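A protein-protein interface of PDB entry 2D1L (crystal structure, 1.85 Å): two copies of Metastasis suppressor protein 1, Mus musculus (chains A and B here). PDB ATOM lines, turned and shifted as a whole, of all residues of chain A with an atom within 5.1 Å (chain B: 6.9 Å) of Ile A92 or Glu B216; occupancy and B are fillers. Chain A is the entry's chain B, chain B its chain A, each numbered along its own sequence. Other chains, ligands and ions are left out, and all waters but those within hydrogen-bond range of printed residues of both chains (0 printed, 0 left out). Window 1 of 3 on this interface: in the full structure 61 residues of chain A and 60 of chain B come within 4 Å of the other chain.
NE2 of His A89 lies within hydrogen-bond range of OE1 of Glu B216, 2.7 Å away.
Ile A92 touches just one residue of chain B: Glu B216.
Glu B216 touches just these residues of chain A: His A89, Ile A92, Ile A223 and Leu A226.
Printed residues of chain A within 4 Å of Ile B217: Ile A223 (3.6 Å) and Leu A226 (3.97 Å).
Of the printed residues of chain B, Leu A226 touches Glu B216 and Ile B217.
Of the printed residues of chain A, Leu B220 touches Ile A223 (3.8 Å).
Of the printed residues of chain B, His A89 touches Ile B213 and Glu B216.
Printed residues of chain A within 4 Å of Ile B213: His A89 (3.4 Å).
Met A219 touches none of the printed residues of chain B.
The nearest printed residue of chain B that does not touch Ile A92 is Ile B213 (7.8 Å).
The nearest printed residue of chain A that does not touch Glu B216 is Arg A88 (7.1 Å).
Among the printed residues, merely in contact across the chains: His A89 with Ile B213 (3.4 Å), Leu A226 with Glu B216 (3.5 Å), Ile A223 with Glu B216 (3.6 Å), Ile A223 with Ile B217 (3.6 Å), Ile A223 with Leu B220 (3.8 Å), Ile A92 with Glu B216 (3.9 Å) and Leu A226 with Ile B217 (3.97 Å).
Positions printed for both chains: 95 and 219.
Hydrophobic or aromatic side chains of chain B that line the printed part of chain A: Ile B213, Ile B217 and Leu B220.
Of the 13 printed residues of chain A, 4 touch a printed residue of chain B.
Among the printed residues, no Asp or Glu carboxylate lies within 4 Å of a Lys or Arg side-chain nitrogen of the other chain.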
ATOM      1  N   ARG A  88      -1.012  -3.124 -16.809  1.00  0.00           N
ATOM      2  CA  ARG A  88      -1.052  -1.829 -16.120  1.00  0.00           C
ATOM      3  C   ARG A  88      -0.278  -0.744 -16.868  1.00  0.00           C
ATOM      4  O   ARG A  88      -0.745   0.397 -16.962  1.00  0.00           O
ATOM      5  CB  ARG A  88      -0.590  -1.930 -14.656  1.00  0.00           C
ATOM      6  CG  ARG A  88      -1.475  -2.829 -13.780  1.00  0.00           C
ATOM      7  CD  ARG A  88      -2.715  -2.133 -13.179  1.00  0.00           C
ATOM      8  NE  ARG A  88      -3.283  -1.118 -14.054  1.00  0.00           N
ATOM      9  CZ  ARG A  88      -4.584  -0.866 -14.183  1.00  0.00           C
ATOM     10  NH1 ARG A  88      -5.484  -1.552 -13.488  1.00  0.00           N
ATOM     11  NH2 ARG A  88      -4.982   0.062 -15.028  1.00  0.00           N
ATOM     12  N   HIS A  89       0.911  -1.077 -17.390  1.00  0.00           N
ATOM     13  CA  HIS A  89       1.639  -0.101 -18.195  1.00  0.00           C
ATOM     14  C   HIS A  89       0.925   0.208 -19.518  1.00  0.00           C
ATOM     15  O   HIS A  89       1.014   1.318 -20.027  1.00  0.00           O
ATOM     16  CB  HIS A  89       3.058  -0.574 -18.446  1.00  0.00           C
ATOM     17  CG  HIS A  89       3.954  -0.339 -17.281  1.00  0.00           C
ATOM     18  ND1 HIS A  89       4.317  -1.341 -16.419  1.00  0.00           N
ATOM     19  CD2 HIS A  89       4.505   0.798 -16.794  1.00  0.00           C
ATOM     20  CE1 HIS A  89       5.085  -0.842 -15.466  1.00  0.00           C
ATOM     21  NE2 HIS A  89       5.205   0.457 -15.665  1.00  0.00           N
ATOM     22  N   ARG A  90       0.235  -0.771 -20.093  1.00  0.00           N
ATOM     23  CA  ARG A  90      -0.541  -0.486 -21.309  1.00  0.00           C
ATOM     24  C   ARG A  90      -1.645   0.549 -21.023  1.00  0.00           C
ATOM     25  O   ARG A  90      -1.989   1.364 -21.886  1.00  0.00           O
ATOM     26  CB  ARG A  90      -1.162  -1.770 -21.854  1.00  0.00           C
ATOM     27  CG  ARG A  90      -1.713  -1.673 -23.238  1.00  0.00           C
ATOM     28  CD  ARG A  90      -0.558  -1.673 -24.249  1.00  0.00           C
ATOM     29  NE  ARG A  90       0.089  -2.972 -24.426  1.00  0.00           N
ATOM     30  CZ  ARG A  90       0.975  -3.197 -25.395  1.00  0.00           C
ATOM     31  NH1 ARG A  90       1.315  -2.199 -26.200  1.00  0.00           N
ATOM     32  NH2 ARG A  90       1.534  -4.382 -25.547  1.00  0.00           N
ATOM     33  N   SER A  91      -2.233   0.501 -19.830  1.00  0.00           N
ATOM     34  CA  SER A  91      -3.264   1.473 -19.469  1.00  0.00           C
ATOM     35  C   SER A  91      -2.616   2.851 -19.372  1.00  0.00           C
ATOM     36  O   SER A  91      -3.167   3.850 -19.830  1.00  0.00           O
ATOM     37  CB  SER A  91      -3.919   1.103 -18.132  1.00  0.00           C
ATOM     38  OG  SER A  91      -4.917   2.049 -17.781  1.00  0.00           O
ATOM     39  N   ILE A  92      -1.436   2.910 -18.768  1.00  0.00           N
ATOM     40  CA  ILE A  92      -0.730   4.174 -18.653  1.00  0.00           C
ATOM     41  C   ILE A  92      -0.408   4.722 -20.037  1.00  0.00           C
ATOM     42  O   ILE A  92      -0.586   5.908 -20.274  1.00  0.00           O
ATOM     43  CB  ILE A  92       0.537   4.056 -17.822  1.00  0.00           C
ATOM     44  CG1 ILE A  92       0.163   3.695 -16.363  1.00  0.00           C
ATOM     45  CG2 ILE A  92       1.328   5.356 -17.874  1.00  0.00           C
ATOM     46  CD1 ILE A  92       1.385   3.170 -15.554  1.00  0.00           C
ATOM     47  N   GLU A  93       0.056   3.852 -20.939  1.00  0.00           N
ATOM     48  CA  GLU A  93       0.303   4.238 -22.347  1.00  0.00           C
ATOM     49  C   GLU A  93      -0.960   4.831 -22.993  1.00  0.00           C
ATOM     50  O   GLU A  93      -0.884   5.809 -23.743  1.00  0.00           O
ATOM     51  CB  GLU A  93       0.775   3.024 -23.156  1.00  0.00           C
ATOM     52  CG  GLU A  93       1.033   3.277 -24.664  1.00  0.00           C
ATOM     53  CD  GLU A  93       0.895   1.996 -25.522  1.00  0.00           C
ATOM     54  OE1 GLU A  93       0.143   2.016 -26.537  1.00  0.00           O
ATOM     55  OE2 GLU A  93       1.535   0.973 -25.179  1.00  0.00           O
ATOM     56  N   ALA A  94      -2.106   4.210 -22.760  1.00  0.00           N
ATOM     57  CA  ALA A  94      -3.339   4.692 -23.379  1.00  0.00           C
ATOM     58  C   ALA A  94      -3.695   6.101 -22.870  1.00  0.00           C
ATOM     59  O   ALA A  94      -4.138   6.965 -23.665  1.00  0.00           O
ATOM     60  CB  ALA A  94      -4.481   3.674 -23.203  1.00  0.00           C
ATOM     61  N   LYS A  95      -3.487   6.360 -21.573  1.00  0.00           N
ATOM     62  CA  LYS A  95      -3.666   7.734 -21.050  1.00  0.00           C
ATOM     63  C   LYS A  95      -2.626   8.728 -21.610  1.00  0.00           C
ATOM     64  O   LYS A  95      -2.919   9.930 -21.762  1.00  0.00           O
ATOM     65  CB  LYS A  95      -3.604   7.754 -19.512  1.00  0.00           C
ATOM     66  CG  LYS A  95      -4.620   6.815 -18.829  1.00  0.00           C
ATOM     67  CD  LYS A  95      -6.048   7.189 -19.109  1.00  0.00           C
ATOM     68  CE  LYS A  95      -6.973   6.302 -18.226  1.00  0.00           C
ATOM     69  NZ  LYS A  95      -8.366   6.226 -18.770  1.00  0.00           N
ATOM     70  N   LEU A  96      -1.404   8.261 -21.874  1.00  0.00           N
ATOM     71  CA  LEU A  96      -0.379   9.148 -22.442  1.00  0.00           C
ATOM     72  C   LEU A  96      -0.806   9.571 -23.847  1.00  0.00           C
ATOM     73  O   LEU A  96      -0.573  10.716 -24.268  1.00  0.00           O
ATOM     74  CB  LEU A  96       1.004   8.455 -22.470  1.00  0.00           C
ATOM     75  CG  LEU A  96       2.188   9.193 -23.107  1.00  0.00           C
ATOM     76  CD1 LEU A  96       2.466  10.528 -22.412  1.00  0.00           C
ATOM     77  CD2 LEU A  96       3.465   8.324 -23.069  1.00  0.00           C
ATOM     78  N   MET A 219      -3.684  10.201 -16.276  1.00  0.00           N
ATOM     79  CA  MET A 219      -2.522   9.354 -16.585  1.00  0.00           C
ATOM     80  C   MET A 219      -1.734   8.989 -15.345  1.00  0.00           C
ATOM     81  O   MET A 219      -1.440   7.815 -15.125  1.00  0.00           O
ATOM     82  CB  MET A 219      -1.598  10.037 -17.587  1.00  0.00           C
ATOM     83  CG  MET A 219      -0.343   9.264 -17.852  1.00  0.00           C
ATOM     84  SD  MET A 219       0.763  10.306 -19.130  1.00  0.00           S
ATOM     85  CE  MET A 219       1.409  11.760 -17.960  1.00  0.00           C
ATOM     86  N   GLU A 222      -3.220   6.286 -12.985  1.00  0.00           N
ATOM     87  CA  GLU A 222      -3.077   4.868 -13.363  1.00  0.00           C
ATOM     88  C   GLU A 222      -1.854   4.213 -12.741  1.00  0.00           C
ATOM     89  O   GLU A 222      -1.769   2.983 -12.647  1.00  0.00           O
ATOM     90  CB  GLU A 222      -2.972   4.713 -14.880  1.00  0.00           C
ATOM     91  CG  GLU A 222      -4.303   4.885 -15.620  1.00  0.00           C
ATOM     92  CD  GLU A 222      -5.385   3.943 -15.104  1.00  0.00           C
ATOM     93  OE1 GLU A 222      -5.307   2.724 -15.383  1.00  0.00           O
ATOM     94  OE2 GLU A 222      -6.315   4.410 -14.407  1.00  0.00           O
ATOM     95  N   ILE A 223      -0.899   5.035 -12.316  1.00  0.00           N
ATOM     96  CA  ILE A 223       0.288   4.512 -11.641  1.00  0.00           C
ATOM     97  C   ILE A 223      -0.049   3.868 -10.288  1.00  0.00           C
ATOM     98  O   ILE A 223       0.757   3.108  -9.735  1.00  0.00           O
ATOM     99  CB  ILE A 223       1.336   5.626 -11.474  1.00  0.00           C
ATOM    100  CG1 ILE A 223       1.812   6.102 -12.849  1.00  0.00           C
ATOM    101  CG2 ILE A 223       2.486   5.187 -10.530  1.00  0.00           C
ATOM    102  CD1 ILE A 223       2.676   7.361 -12.776  1.00  0.00           C
ATOM    103  N   LEU A 226       0.518   0.052  -9.882  1.00  0.00           N
ATOM    104  CA  LEU A 226       1.856  -0.571  -9.947  1.00  0.00           C
ATOM    105  C   LEU A 226       2.392  -1.110  -8.619  1.00  0.00           C
ATOM    106  O   LEU A 226       3.068  -2.140  -8.596  1.00  0.00           O
ATOM    107  CB  LEU A 226       2.859   0.397 -10.564  1.00  0.00           C
ATOM    108  CG  LEU A 226       2.499   0.887 -11.963  1.00  0.00           C
ATOM    109  CD1 LEU A 226       3.713   1.660 -12.478  1.00  0.00           C
ATOM    110  CD2 LEU A 226       2.190  -0.286 -12.867  1.00  0.00           C
ATOM    111  N   LYS B  95      11.332  13.915 -12.050  1.00  0.00           N
ATOM    112  CA  LYS B  95      11.043  12.534 -11.764  1.00  0.00           C
ATOM    113  C   LYS B  95      11.109  11.729 -13.047  1.00  0.00           C
ATOM    114  O   LYS B  95      11.604  10.587 -13.055  1.00  0.00           O
ATOM    115  CB  LYS B  95       9.690  12.402 -11.068  1.00  0.00           C
ATOM    116  CG  LYS B  95       9.781  12.736  -9.570  1.00  0.00           C
ATOM    117  CD  LYS B  95       8.464  12.567  -8.901  1.00  0.00           C
ATOM    118  CE  LYS B  95       8.592  12.928  -7.400  1.00  0.00           C
ATOM    119  NZ  LYS B  95       7.276  13.184  -6.821  1.00  0.00           N
ATOM    120  N   PHE B  99      13.522   8.550 -13.749  1.00  0.00           N
ATOM    121  CA  PHE B  99      12.994   7.309 -14.330  1.00  0.00           C
ATOM    122  C   PHE B  99      13.847   6.885 -15.547  1.00  0.00           C
ATOM    123  O   PHE B  99      14.225   5.734 -15.676  1.00  0.00           O
ATOM    124  CB  PHE B  99      11.535   7.495 -14.788  1.00  0.00           C
ATOM    125  CG  PHE B  99      10.963   6.301 -15.493  1.00  0.00           C
ATOM    126  CD1 PHE B  99      10.423   5.243 -14.776  1.00  0.00           C
ATOM    127  CD2 PHE B  99      10.965   6.236 -16.882  1.00  0.00           C
ATOM    128  CE1 PHE B  99       9.887   4.148 -15.413  1.00  0.00           C
ATOM    129  CE2 PHE B  99      10.441   5.122 -17.549  1.00  0.00           C
ATOM    130  CZ  PHE B  99       9.893   4.083 -16.824  1.00  0.00           C
ATOM    131  N   PRO B 211      13.485  -1.197  -9.171  1.00  0.00           N
ATOM    132  CA  PRO B 211      13.826   0.226  -8.938  1.00  0.00           C
ATOM    133  C   PRO B 211      13.387   1.178 -10.059  1.00  0.00           C
ATOM    134  O   PRO B 211      13.158   2.368  -9.796  1.00  0.00           O
ATOM    135  CB  PRO B 211      15.359   0.234  -8.801  1.00  0.00           C
ATOM    136  CG  PRO B 211      15.816  -1.042  -9.354  1.00  0.00           C
ATOM    137  CD  PRO B 211      14.683  -2.039  -9.309  1.00  0.00           C
ATOM    138  N   VAL B 212      13.265   0.671 -11.286  1.00  0.00           N
ATOM    139  CA  VAL B 212      12.713   1.495 -12.360  1.00  0.00           C
ATOM    140  C   VAL B 212      11.243   1.824 -12.086  1.00  0.00           C
ATOM    141  O   VAL B 212      10.807   2.983 -12.126  1.00  0.00           O
ATOM    142  CB  VAL B 212      12.882   0.793 -13.752  1.00  0.00           C
ATOM    143  CG1 VAL B 212      12.359   1.710 -14.873  1.00  0.00           C
ATOM    144  CG2 VAL B 212      14.350   0.427 -13.990  1.00  0.00           C
ATOM    145  N   ILE B 213      10.483   0.799 -11.752  1.00  0.00           N
ATOM    146  CA  ILE B 213       9.085   1.011 -11.375  1.00  0.00           C
ATOM    147  C   ILE B 213       8.926   1.920 -10.145  1.00  0.00           C
ATOM    148  O   ILE B 213       7.985   2.731 -10.081  1.00  0.00           O
ATOM    149  CB  ILE B 213       8.366  -0.352 -11.203  1.00  0.00           C
ATOM    150  CG1 ILE B 213       8.499  -1.183 -12.489  1.00  0.00           C
ATOM    151  CG2 ILE B 213       6.924  -0.135 -10.753  1.00  0.00           C
ATOM    152  CD1 ILE B 213       7.992  -0.516 -13.732  1.00  0.00           C
ATOM    153  N   GLU B 214       9.819   1.809  -9.159  1.00  0.00           N
ATOM    154  CA  GLU B 214       9.806   2.742  -8.044  1.00  0.00           C
ATOM    155  C   GLU B 214       9.838   4.212  -8.456  1.00  0.00           C
ATOM    156  O   GLU B 214       9.166   5.040  -7.846  1.00  0.00           O
ATOM    157  CB  GLU B 214      10.922   2.465  -7.010  1.00  0.00           C
ATOM    158  CG  GLU B 214      10.803   3.411  -5.751  1.00  0.00           C
ATOM    159  CD  GLU B 214       9.355   3.513  -5.155  1.00  0.00           C
ATOM    160  OE1 GLU B 214       8.791   2.445  -4.785  1.00  0.00           O
ATOM    161  OE2 GLU B 214       8.772   4.652  -5.037  1.00  0.00           O
ATOM    162  N   GLU B 215      10.617   4.558  -9.476  1.00  0.00           N
ATOM    163  CA  GLU B 215      10.696   5.959  -9.905  1.00  0.00           C
ATOM    164  C   GLU B 215       9.361   6.392 -10.508  1.00  0.00           C
ATOM    165  O   GLU B 215       8.910   7.519 -10.315  1.00  0.00           O
ATOM    166  CB  GLU B 215      11.841   6.193 -10.904  1.00  0.00           C
ATOM    167  CG  GLU B 215      13.195   5.838 -10.327  1.00  0.00           C
ATOM    168  CD  GLU B 215      13.549   6.660  -9.108  1.00  0.00           C
ATOM    169  OE1 GLU B 215      13.067   7.807  -8.980  1.00  0.00           O
ATOM    170  OE2 GLU B 215      14.314   6.159  -8.263  1.00  0.00           O
ATOM    171  N   GLU B 216       8.699   5.458 -11.180  1.00  0.00           N
ATOM    172  CA  GLU B 216       7.379   5.721 -11.731  1.00  0.00           C
ATOM    173  C   GLU B 216       6.351   5.947 -10.609  1.00  0.00           C
ATOM    174  O   GLU B 216       5.606   6.930 -10.626  1.00  0.00           O
ATOM    175  CB  GLU B 216       6.992   4.540 -12.626  1.00  0.00           C
ATOM    176  CG  GLU B 216       5.903   4.812 -13.607  1.00  0.00           C
ATOM    177  CD  GLU B 216       5.826   3.710 -14.683  1.00  0.00           C
ATOM    178  OE1 GLU B 216       6.382   2.602 -14.459  1.00  0.00           O
ATOM    179  OE2 GLU B 216       5.230   3.976 -15.745  1.00  0.00           O
ATOM    180  N   ILE B 217       6.333   5.052  -9.635  1.00  0.00           N
ATOM    181  CA  ILE B 217       5.442   5.146  -8.483  1.00  0.00           C
ATOM    182  C   ILE B 217       5.633   6.479  -7.721  1.00  0.00           C
ATOM    183  O   ILE B 217       4.665   7.001  -7.132  1.00  0.00           O
ATOM    184  CB  ILE B 217       5.659   3.944  -7.541  1.00  0.00           C
ATOM    185  CG1 ILE B 217       5.083   2.676  -8.191  1.00  0.00           C
ATOM    186  CG2 ILE B 217       5.044   4.172  -6.164  1.00  0.00           C
ATOM    187  CD1 ILE B 217       5.567   1.391  -7.622  1.00  0.00           C
ATOM    188  N   SER B 218       6.849   7.037  -7.739  1.00  0.00           N
ATOM    189  CA  SER B 218       7.101   8.289  -7.008  1.00  0.00           C
ATOM    190  C   SER B 218       6.304   9.456  -7.584  1.00  0.00           C
ATOM    191  O   SER B 218       6.168  10.498  -6.944  1.00  0.00           O
ATOM    192  CB  SER B 218       8.597   8.644  -6.962  1.00  0.00           C
ATOM    193  OG  SER B 218       9.094   9.052  -8.229  1.00  0.00           O
ATOM    194  N   MET B 219       5.783   9.281  -8.787  1.00  0.00           N
ATOM    195  CA  MET B 219       5.000  10.345  -9.411  1.00  0.00           C
ATOM    196  C   MET B 219       3.601  10.511  -8.844  1.00  0.00           C
ATOM    197  O   MET B 219       2.938  11.510  -9.122  1.00  0.00           O
ATOM    198  CB  MET B 219       4.946  10.110 -10.915  1.00  0.00           C
ATOM    199  CG  MET B 219       6.333  10.125 -11.510  1.00  0.00           C
ATOM    200  SD  MET B 219       6.193   9.697 -13.404  1.00  0.00           S
ATOM    201  CE  MET B 219       8.134   9.401 -13.851  1.00  0.00           C
ATOM    202  N   LEU B 220       3.158   9.557  -8.036  1.00  0.00           N
ATOM    203  CA  LEU B 220       1.830   9.688  -7.406  1.00  0.00           C
ATOM    204  C   LEU B 220       1.752  10.897  -6.477  1.00  0.00           C
ATOM    205  O   LEU B 220       0.685  11.515  -6.336  1.00  0.00           O
ATOM    206  CB  LEU B 220       1.478   8.402  -6.649  1.00  0.00           C
ATOM    207  CG  LEU B 220       1.191   7.202  -7.563  1.00  0.00           C
ATOM    208  CD1 LEU B 220       1.085   5.958  -6.671  1.00  0.00           C
ATOM    209  CD2 LEU B 220      -0.136   7.402  -8.299  1.00  0.00           C
